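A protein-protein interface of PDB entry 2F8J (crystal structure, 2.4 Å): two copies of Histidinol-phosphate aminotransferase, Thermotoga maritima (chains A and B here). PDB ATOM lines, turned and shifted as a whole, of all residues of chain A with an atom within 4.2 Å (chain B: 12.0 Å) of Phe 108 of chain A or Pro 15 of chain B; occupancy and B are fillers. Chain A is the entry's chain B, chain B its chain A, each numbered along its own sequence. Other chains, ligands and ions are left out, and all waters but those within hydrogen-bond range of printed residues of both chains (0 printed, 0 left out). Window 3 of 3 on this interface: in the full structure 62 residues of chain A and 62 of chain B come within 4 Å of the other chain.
Of the 12 printed residues of chain A, 4 touch a printed residue of chain B. Printed residues of chain A that touch a printed residue of chain B: Leu 106, Met 107, Phe 108 and Glu 150. Hydrophobic or aromatic side chains of chain A that line the printed part of chain B: Leu 106, Met 107 and Phe 108. Of the 20 printed residues of chain B, 5 touch a printed residue of chain A. Hydrophobic or aromatic side chains of chain B that line the printed part of chain A: Pro 15, Ile 19, Tyr 102 and Leu 106.
Leu 106 of chain A touches Tyr 102 of chain B (CD1 to OH, 3.2 Å). Leu 106 of chain B touches Leu 106 of chain A (CD2 to CD2, 3.5 Å). Ile 19 of chain B touches Met 107 of chain A. CD2 of Phe 108 of chain A touches CG of Pro 15 of chain B, 3.6 Å away. Glu 150 of chain A touches Asn 14 of chain B (OE2 to CB, 3.1 Å).
Leu 106 of chain A touches its own counterpart, Leu 106 of chain B. 1 position is printed for both chains. Of the 5 pairs that touch across the chains among the printed residues, 1 has its exchanged pair printed and touching as well.
OD1 of Asn 14 of chain B sits close to N of Leu 16 of chain B (3.2 Å). The side-chain amide nitrogen (ND2) of Asn 14 of chain B lies within hydrogen-bond range of the side-chain carboxylate (OD2) of Asp 17 of chain B (2.7 Å).
Of chain B, only Pro 15 comes within 4 Å of Phe 108 of chain A. Of chain A, only Phe 108 (3.6 Å) comes within 4 Å of Pro 15 of chain B. No residue of chain B comes within 4 Å of Met 104 of chain A. Printed residues of chain B within 4 Å of Met 107 of chain A: Ile 19. No residue of chain B comes within 4 Å of Asp 109 of chain A. Glu 150 of chain A touches one residue of chain B. No residue of chain B comes within 4 Å of Gly 151 of chain A. Val 153 of chain A touches none of the printed residues of chain B. No residue of chain B comes within 4 Å of Phe 181 of chain A. Of the printed residues of chain A, Ile 19 of chain B touches Met 107 (3.6 Å). Of the printed residues of chain B, Leu 106 of chain A touches Tyr 102 (3.2 Å) and Leu 106 (3.5 Å). Arg 22 of chain B touches none of the printed residues of chain A. Ala 20 of chain B touches none of the printed residues of chain A. The nearest residue of chain A that does not touch Pro 15 of chain B is Met 107 of chain A (4.04 Å).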
ATOM      1  N   MET A 104      -6.885   6.531   8.700  1.00  0.00           N
ATOM      2  CA  MET A 104      -6.724   7.676   7.811  1.00  0.00           C
ATOM      3  C   MET A 104      -5.562   8.566   8.235  1.00  0.00           C
ATOM      4  O   MET A 104      -4.820   9.029   7.389  1.00  0.00           O
ATOM      5  CB  MET A 104      -8.028   8.465   7.673  1.00  0.00           C
ATOM      6  CG  MET A 104      -9.050   7.768   6.801  1.00  0.00           C
ATOM      7  SD  MET A 104     -10.654   8.564   6.679  1.00  0.00           S
ATOM      8  CE  MET A 104     -10.415   9.527   5.191  1.00  0.00           C
ATOM      9  N   MET A 105      -5.379   8.789   9.525  1.00  0.00           N
ATOM     10  CA  MET A 105      -4.214   9.566   9.971  1.00  0.00           C
ATOM     11  C   MET A 105      -2.866   8.909   9.657  1.00  0.00           C
ATOM     12  O   MET A 105      -1.903   9.614   9.467  1.00  0.00           O
ATOM     13  CB  MET A 105      -4.312   9.910  11.445  1.00  0.00           C
ATOM     14  CG  MET A 105      -5.470  10.806  11.721  1.00  0.00           C
ATOM     15  SD  MET A 105      -5.530  11.431  13.385  1.00  0.00           S
ATOM     16  CE  MET A 105      -6.858  12.616  13.181  1.00  0.00           C
ATOM     17  N   LEU A 106      -2.829   7.581   9.583  1.00  0.00           N
ATOM     18  CA  LEU A 106      -1.647   6.846   9.145  1.00  0.00           C
ATOM     19  C   LEU A 106      -1.431   6.932   7.618  1.00  0.00           C
ATOM     20  O   LEU A 106      -0.332   6.690   7.133  1.00  0.00           O
ATOM     21  CB  LEU A 106      -1.749   5.362   9.576  1.00  0.00           C
ATOM     22  CG  LEU A 106      -1.726   5.047  11.087  1.00  0.00           C
ATOM     23  CD1 LEU A 106      -2.179   3.625  11.386  1.00  0.00           C
ATOM     24  CD2 LEU A 106      -0.344   5.283  11.667  1.00  0.00           C
ATOM     25  N   MET A 107      -2.480   7.274   6.868  1.00  0.00           N
ATOM     26  CA  MET A 107      -2.463   7.173   5.414  1.00  0.00           C
ATOM     27  C   MET A 107      -1.941   8.412   4.722  1.00  0.00           C
ATOM     28  O   MET A 107      -1.306   8.301   3.683  1.00  0.00           O
ATOM     29  CB  MET A 107      -3.864   6.895   4.888  1.00  0.00           C
ATOM     30  CG  MET A 107      -4.410   5.509   5.252  1.00  0.00           C
ATOM     31  SD  MET A 107      -5.849   5.053   4.250  1.00  0.00           S
ATOM     32  CE  MET A 107      -7.191   5.649   5.156  1.00  0.00           C
ATOM     33  N   PHE A 108      -2.211   9.589   5.280  1.00  0.00           N
ATOM     34  CA  PHE A 108      -1.864  10.861   4.631  1.00  0.00           C
ATOM     35  C   PHE A 108      -0.680  11.550   5.319  1.00  0.00           C
ATOM     36  O   PHE A 108      -0.334  11.235   6.454  1.00  0.00           O
ATOM     37  CB  PHE A 108      -3.071  11.793   4.607  1.00  0.00           C
ATOM     38  CG  PHE A 108      -4.231  11.259   3.799  1.00  0.00           C
ATOM     39  CD1 PHE A 108      -5.114  10.352   4.346  1.00  0.00           C
ATOM     40  CD2 PHE A 108      -4.424  11.657   2.483  1.00  0.00           C
ATOM     41  CE1 PHE A 108      -6.173   9.843   3.584  1.00  0.00           C
ATOM     42  CE2 PHE A 108      -5.472  11.153   1.728  1.00  0.00           C
ATOM     43  CZ  PHE A 108      -6.341  10.255   2.269  1.00  0.00           C
ATOM     44  N   ASP A 109      -0.065  12.495   4.611  1.00  0.00           N
ATOM     45  CA  ASP A 109       1.096  13.219   5.109  1.00  0.00           C
ATOM     46  C   ASP A 109       0.749  14.125   6.291  1.00  0.00           C
ATOM     47  O   ASP A 109       1.563  14.283   7.189  1.00  0.00           O
ATOM     48  CB  ASP A 109       1.741  14.087   4.015  1.00  0.00           C
ATOM     49  CG  ASP A 109       2.563  13.279   3.001  1.00  0.00           C
ATOM     50  OD1 ASP A 109       3.689  12.801   3.332  1.00  0.00           O
ATOM     51  OD2 ASP A 109       2.094  13.154   1.841  1.00  0.00           O
ATOM     52  N   ARG A 110      -0.433  14.737   6.268  1.00  0.00           N
ATOM     53  CA  ARG A 110      -0.822  15.675   7.302  1.00  0.00           C
ATOM     54  C   ARG A 110      -2.307  15.623   7.532  1.00  0.00           C
ATOM     55  O   ARG A 110      -3.061  15.471   6.591  1.00  0.00           O
ATOM     56  CB  ARG A 110      -0.409  17.089   6.917  1.00  0.00           C
ATOM     57  CG  ARG A 110      -0.712  18.127   7.988  1.00  0.00           C
ATOM     58  CD  ARG A 110      -0.216  19.507   7.625  1.00  0.00           C
ATOM     59  NE  ARG A 110      -0.937  20.090   6.492  1.00  0.00           N
ATOM     60  CZ  ARG A 110      -0.879  21.372   6.137  1.00  0.00           C
ATOM     61  NH1 ARG A 110      -0.164  22.252   6.829  1.00  0.00           N
ATOM     62  NH2 ARG A 110      -1.576  21.792   5.095  1.00  0.00           N
ATOM     63  N   GLU A 150      -3.156  18.463  -1.847  1.00  0.00           N
ATOM     64  CA  GLU A 150      -2.875  17.036  -1.929  1.00  0.00           C
ATOM     65  C   GLU A 150      -1.797  16.649  -0.904  1.00  0.00           C
ATOM     66  O   GLU A 150      -0.845  17.392  -0.694  1.00  0.00           O
ATOM     67  CB  GLU A 150      -2.455  16.643  -3.348  1.00  0.00           C
ATOM     68  CG  GLU A 150      -2.564  15.151  -3.587  1.00  0.00           C
ATOM     69  CD  GLU A 150      -2.304  14.745  -5.025  1.00  0.00           C
ATOM     70  OE1 GLU A 150      -1.144  14.883  -5.488  1.00  0.00           O
ATOM     71  OE2 GLU A 150      -3.268  14.263  -5.675  1.00  0.00           O
ATOM     72  N   GLY A 151      -1.977  15.514  -0.238  1.00  0.00           N
ATOM     73  CA  GLY A 151      -1.137  15.140   0.901  1.00  0.00           C
ATOM     74  C   GLY A 151      -1.831  15.327   2.246  1.00  0.00           C
ATOM     75  O   GLY A 151      -1.485  14.663   3.210  1.00  0.00           O
ATOM     76  N   ASP A 152      -2.796  16.244   2.311  1.00  0.00           N
ATOM     77  CA  ASP A 152      -3.582  16.502   3.526  1.00  0.00           C
ATOM     78  C   ASP A 152      -4.852  15.690   3.549  1.00  0.00           C
ATOM     79  O   ASP A 152      -5.476  15.499   2.510  1.00  0.00           O
ATOM     80  CB  ASP A 152      -3.992  17.983   3.597  1.00  0.00           C
ATOM     81  CG  ASP A 152      -2.799  18.932   3.553  1.00  0.00           C
ATOM     82  OD1 ASP A 152      -1.734  18.573   4.072  1.00  0.00           O
ATOM     83  OD2 ASP A 152      -2.923  20.048   3.003  1.00  0.00           O
ATOM     84  N   VAL A 153      -5.260  15.261   4.742  1.00  0.00           N
ATOM     85  CA  VAL A 153      -6.654  14.834   4.985  1.00  0.00           C
ATOM     86  C   VAL A 153      -7.242  15.836   5.964  1.00  0.00           C
ATOM     87  O   VAL A 153      -6.617  16.164   6.948  1.00  0.00           O
ATOM     88  CB  VAL A 153      -6.803  13.340   5.450  1.00  0.00           C
ATOM     89  CG1 VAL A 153      -5.885  12.996   6.595  1.00  0.00           C
ATOM     90  CG2 VAL A 153      -8.220  13.024   5.812  1.00  0.00           C
ATOM     91  N   PHE A 181      -7.790  15.812   0.690  1.00  0.00           N
ATOM     92  CA  PHE A 181      -8.740  14.733   0.912  1.00  0.00           C
ATOM     93  C   PHE A 181      -9.635  15.113   2.105  1.00  0.00           C
ATOM     94  O   PHE A 181      -9.143  15.398   3.197  1.00  0.00           O
ATOM     95  CB  PHE A 181      -8.020  13.409   1.168  1.00  0.00           C
ATOM     96  CG  PHE A 181      -8.903  12.211   1.001  1.00  0.00           C
ATOM     97  CD1 PHE A 181      -9.698  11.767   2.043  1.00  0.00           C
ATOM     98  CD2 PHE A 181      -8.980  11.554  -0.210  1.00  0.00           C
ATOM     99  CE1 PHE A 181     -10.523  10.678   1.885  1.00  0.00           C
ATOM    100  CE2 PHE A 181      -9.818  10.463  -0.376  1.00  0.00           C
ATOM    101  CZ  PHE A 181     -10.588  10.033   0.662  1.00  0.00           C
ATOM    102  N   HIS B  12       5.111  13.743  -7.204  1.00  0.00           N
ATOM    103  CA  HIS B  12       4.502  13.184  -8.452  1.00  0.00           C
ATOM    104  C   HIS B  12       3.718  11.876  -8.212  1.00  0.00           C
ATOM    105  O   HIS B  12       3.604  11.041  -9.118  1.00  0.00           O
ATOM    106  CB  HIS B  12       5.591  12.965  -9.515  1.00  0.00           C
ATOM    107  N   MET B  13       3.192  11.707  -6.998  1.00  0.00           N
ATOM    108  CA  MET B  13       2.335  10.567  -6.643  1.00  0.00           C
ATOM    109  C   MET B  13       1.429  10.981  -5.482  1.00  0.00           C
ATOM    110  O   MET B  13       1.927  11.364  -4.423  1.00  0.00           O
ATOM    111  CB  MET B  13       3.170   9.344  -6.212  1.00  0.00           C
ATOM    112  CG  MET B  13       3.869   8.587  -7.338  1.00  0.00           C
ATOM    113  N   ASN B  14       0.111  10.907  -5.679  1.00  0.00           N
ATOM    114  CA  ASN B  14      -0.836  11.160  -4.588  1.00  0.00           C
ATOM    115  C   ASN B  14      -0.756  10.037  -3.546  1.00  0.00           C
ATOM    116  O   ASN B  14      -0.359   8.917  -3.874  1.00  0.00           O
ATOM    117  CB  ASN B  14      -2.261  11.382  -5.136  1.00  0.00           C
ATOM    118  CG  ASN B  14      -3.009  10.092  -5.430  1.00  0.00           C
ATOM    119  OD1 ASN B  14      -3.687   9.537  -4.560  1.00  0.00           O
ATOM    120  ND2 ASN B  14      -2.941   9.644  -6.675  1.00  0.00           N
ATOM    121  N   PRO B  15      -1.114  10.333  -2.281  1.00  0.00           N
ATOM    122  CA  PRO B  15      -0.812   9.392  -1.179  1.00  0.00           C
ATOM    123  C   PRO B  15      -1.451   7.998  -1.303  1.00  0.00           C
ATOM    124  O   PRO B  15      -0.927   7.038  -0.739  1.00  0.00           O
ATOM    125  CB  PRO B  15      -1.333  10.121   0.073  1.00  0.00           C
ATOM    126  CG  PRO B  15      -2.317  11.125  -0.449  1.00  0.00           C
ATOM    127  CD  PRO B  15      -1.832  11.532  -1.803  1.00  0.00           C
ATOM    128  N   LEU B  16      -2.559   7.904  -2.031  1.00  0.00           N
ATOM    129  CA  LEU B  16      -3.207   6.619  -2.311  1.00  0.00           C
ATOM    130  C   LEU B  16      -2.393   5.727  -3.259  1.00  0.00           C
ATOM    131  O   LEU B  16      -2.478   4.501  -3.180  1.00  0.00           O
ATOM    132  CB  LEU B  16      -4.610   6.843  -2.893  1.00  0.00           C
ATOM    133  CG  LEU B  16      -5.562   7.707  -2.059  1.00  0.00           C
ATOM    134  CD1 LEU B  16      -6.941   7.799  -2.708  1.00  0.00           C
ATOM    135  CD2 LEU B  16      -5.656   7.179  -0.634  1.00  0.00           C
ATOM    136  N   ASP B  17      -1.638   6.346  -4.169  1.00  0.00           N
ATOM    137  CA  ASP B  17      -0.740   5.608  -5.055  1.00  0.00           C
ATOM    138  C   ASP B  17       0.485   5.143  -4.293  1.00  0.00           C
ATOM    139  O   ASP B  17       0.994   4.069  -4.569  1.00  0.00           O
ATOM    140  CB  ASP B  17      -0.277   6.460  -6.231  1.00  0.00           C
ATOM    141  CG  ASP B  17      -1.404   6.858  -7.153  1.00  0.00           C
ATOM    142  OD1 ASP B  17      -2.444   6.152  -7.180  1.00  0.00           O
ATOM    143  OD2 ASP B  17      -1.240   7.893  -7.849  1.00  0.00           O
ATOM    144  N   LEU B  18       0.957   5.947  -3.344  1.00  0.00           N
ATOM    145  CA  LEU B  18       2.119   5.579  -2.547  1.00  0.00           C
ATOM    146  C   LEU B  18       1.802   4.335  -1.693  1.00  0.00           C
ATOM    147  O   LEU B  18       2.577   3.360  -1.682  1.00  0.00           O
ATOM    148  CB  LEU B  18       2.594   6.760  -1.682  1.00  0.00           C
ATOM    149  CG  LEU B  18       2.916   8.082  -2.414  1.00  0.00           C
ATOM    150  CD1 LEU B  18       3.155   9.239  -1.452  1.00  0.00           C
ATOM    151  CD2 LEU B  18       4.113   7.933  -3.341  1.00  0.00           C
ATOM    152  N   ILE B  19       0.654   4.358  -1.011  1.00  0.00           N
ATOM    153  CA  ILE B  19       0.166   3.202  -0.262  1.00  0.00           C
ATOM    154  C   ILE B  19       0.088   1.950  -1.142  1.00  0.00           C
ATOM    155  O   ILE B  19       0.585   0.895  -0.754  1.00  0.00           O
ATOM    156  CB  ILE B  19      -1.218   3.493   0.405  1.00  0.00           C
ATOM    157  CG1 ILE B  19      -1.055   4.483   1.565  1.00  0.00           C
ATOM    158  CG2 ILE B  19      -1.871   2.215   0.947  1.00  0.00           C
ATOM    159  CD1 ILE B  19      -2.251   5.392   1.779  1.00  0.00           C
ATOM    160  N   ALA B  20      -0.516   2.074  -2.323  1.00  0.00           N
ATOM    161  CA  ALA B  20      -0.635   0.950  -3.250  1.00  0.00           C
ATOM    162  C   ALA B  20       0.737   0.383  -3.663  1.00  0.00           C
ATOM    163  O   ALA B  20       0.871  -0.819  -3.932  1.00  0.00           O
ATOM    164  CB  ALA B  20      -1.442   1.360  -4.491  1.00  0.00           C
ATOM    165  N   LYS B  21       1.742   1.262  -3.704  1.00  0.00           N
ATOM    166  CA  LYS B  21       3.114   0.876  -4.027  1.00  0.00           C
ATOM    167  C   LYS B  21       3.749   0.114  -2.868  1.00  0.00           C
ATOM    168  O   LYS B  21       4.325  -0.949  -3.067  1.00  0.00           O
ATOM    169  CB  LYS B  21       3.975   2.106  -4.385  1.00  0.00           C
ATOM    170  N   ARG B  22       3.644   0.650  -1.662  1.00  0.00           N
ATOM    171  CA  ARG B  22       4.411   0.108  -0.545  1.00  0.00           C
ATOM    172  C   ARG B  22       3.706  -1.050   0.163  1.00  0.00           C
ATOM    173  O   ARG B  22       4.357  -1.964   0.644  1.00  0.00           O
ATOM    174  CB  ARG B  22       4.787   1.220   0.453  1.00  0.00           C
ATOM    175  CG  ARG B  22       3.642   1.699   1.360  1.00  0.00           C
ATOM    176  CD  ARG B  22       3.838   3.150   1.776  1.00  0.00           C
ATOM    177  NE  ARG B  22       2.701   3.698   2.523  1.00  0.00           N
ATOM    178  CZ  ARG B  22       2.470   3.492   3.814  1.00  0.00           C
ATOM    179  NH1 ARG B  22       3.286   2.727   4.519  1.00  0.00           N
ATOM    180  NH2 ARG B  22       1.418   4.050   4.409  1.00  0.00           N
ATOM    181  N   ALA B  23       2.379  -1.026   0.219  1.00  0.00           N
ATOM    182  CA  ALA B  23       1.655  -1.984   1.046  1.00  0.00           C
ATOM    183  C   ALA B  23       1.087  -3.137   0.224  1.00  0.00           C
ATOM    184  O   ALA B  23       0.636  -2.943  -0.890  1.00  0.00           O
ATOM    185  CB  ALA B  23       0.554  -1.272   1.818  1.00  0.00           C
ATOM    186  N   TYR B  24       1.121  -4.339   0.793  1.00  0.00           N
ATOM    187  CA  TYR B  24       0.536  -5.518   0.164  1.00  0.00           C
ATOM    188  C   TYR B  24      -0.987  -5.367  -0.043  1.00  0.00           C
ATOM    189  O   TYR B  24      -1.683  -4.732   0.756  1.00  0.00           O
ATOM    190  CB  TYR B  24       0.794  -6.764   1.010  1.00  0.00           C
ATOM    191  CG  TYR B  24       2.242  -7.182   1.142  1.00  0.00           C
ATOM    192  CD1 TYR B  24       3.040  -6.711   2.189  1.00  0.00           C
ATOM    193  CD2 TYR B  24       2.808  -8.085   0.245  1.00  0.00           C
ATOM    194  CE1 TYR B  24       4.363  -7.107   2.326  1.00  0.00           C
ATOM    195  CE2 TYR B  24       4.138  -8.489   0.372  1.00  0.00           C
ATOM    196  CZ  TYR B  24       4.907  -7.999   1.418  1.00  0.00           C
ATOM    197  OH  TYR B  24       6.223  -8.402   1.539  1.00  0.00           O
ATOM    198  N   TYR B 102       0.748  -4.256  15.882  1.00  0.00           N
ATOM    199  CA  TYR B 102       0.570  -3.096  15.021  1.00  0.00           C
ATOM    200  C   TYR B 102       0.867  -1.793  15.779  1.00  0.00           C
ATOM    201  O   TYR B 102       1.620  -0.937  15.305  1.00  0.00           O
ATOM    202  CB  TYR B 102      -0.861  -3.138  14.494  1.00  0.00           C
ATOM    203  CG  TYR B 102      -1.290  -2.152  13.424  1.00  0.00           C
ATOM    204  CD1 TYR B 102      -1.717  -0.869  13.765  1.00  0.00           C
ATOM    205  CD2 TYR B 102      -1.392  -2.535  12.090  1.00  0.00           C
ATOM    206  CE1 TYR B 102      -2.166   0.031  12.792  1.00  0.00           C
ATOM    207  CE2 TYR B 102      -1.860  -1.640  11.099  1.00  0.00           C
ATOM    208  CZ  TYR B 102      -2.248  -0.354  11.464  1.00  0.00           C
ATOM    209  OH  TYR B 102      -2.724   0.555  10.529  1.00  0.00           O
ATOM    210  N   LEU B 106       3.952   1.324  15.836  1.00  0.00           N
ATOM    211  CA  LEU B 106       3.766   2.773  15.893  1.00  0.00           C
ATOM    212  C   LEU B 106       4.526   3.408  17.047  1.00  0.00           C
ATOM    213  O   LEU B 106       4.765   4.590  17.022  1.00  0.00           O
ATOM    214  CB  LEU B 106       2.283   3.151  16.058  1.00  0.00           C
ATOM    215  CG  LEU B 106       1.287   2.625  15.043  1.00  0.00           C
ATOM    216  CD1 LEU B 106      -0.125   3.005  15.465  1.00  0.00           C
ATOM    217  CD2 LEU B 106       1.616   3.165  13.661  1.00  0.00           C
ATOM    218  N   LYS B 126       5.228  -2.473   6.669  1.00  0.00           N
ATOM    219  CA  LYS B 126       5.025  -1.810   5.378  1.00  0.00           C
ATOM    220  C   LYS B 126       3.695  -1.057   5.328  1.00  0.00           C
ATOM    221  O   LYS B 126       3.625   0.023   4.754  1.00  0.00           O
ATOM    222  CB  LYS B 126       5.101  -2.795   4.206  1.00  0.00           C
ATOM    223  CG  LYS B 126       6.506  -3.297   3.859  1.00  0.00           C
ATOM    224  CD  LYS B 126       6.475  -4.293   2.691  1.00  0.00           C
ATOM    225  N   ALA B 127       2.647  -1.631   5.913  1.00  0.00           N
ATOM    226  CA  ALA B 127       1.326  -0.965   5.960  1.00  0.00           C
ATOM    227  C   ALA B 127       1.412   0.419   6.598  1.00  0.00           C
ATOM    228  O   ALA B 127       0.936   1.397   6.026  1.00  0.00           O
ATOM    229  CB  ALA B 127       0.303  -1.810   6.711  1.00  0.00           C
ATOM    230  N   VAL B 128       2.026   0.491   7.777  1.00  0.00           N
ATOM    231  CA  VAL B 128       2.102   1.731   8.544  1.00  0.00           C
ATOM    232  C   VAL B 128       3.362   2.577   8.236  1.00  0.00           C
ATOM    233  O   VAL B 128       3.539   3.637   8.826  1.00  0.00           O
ATOM    234  CB  VAL B 128       1.996   1.426  10.054  1.00  0.00           C
ATOM    235  CG1 VAL B 128       0.778   0.498  10.325  1.00  0.00           C
ATOM    236  CG2 VAL B 128       3.300   0.805  10.605  1.00  0.00           C
ATOM    237  N   GLY B 129       4.218   2.109   7.324  1.00  0.00           N
ATOM    238  CA  GLY B 129       5.447   2.828   6.976  1.00  0.00           C
ATOM    239  C   GLY B 129       6.475   2.871   8.098  1.00  0.00           C
ATOM    240  O   GLY B 129       7.220   3.843   8.242  1.00  0.00           O
ATOM    241  N   ALA B 130       6.522   1.811   8.899  1.00  0.00           N
ATOM    242  CA  ALA B 130       7.526   1.684   9.952  1.00  0.00           C
ATOM    243  C   ALA B 130       8.905   1.388   9.362  1.00  0.00           C
ATOM    244  O   ALA B 130       9.010   0.677   8.376  1.00  0.00           O
ATOM    245  CB  ALA B 130       7.105   0.580  10.906  1.00  0.00           C
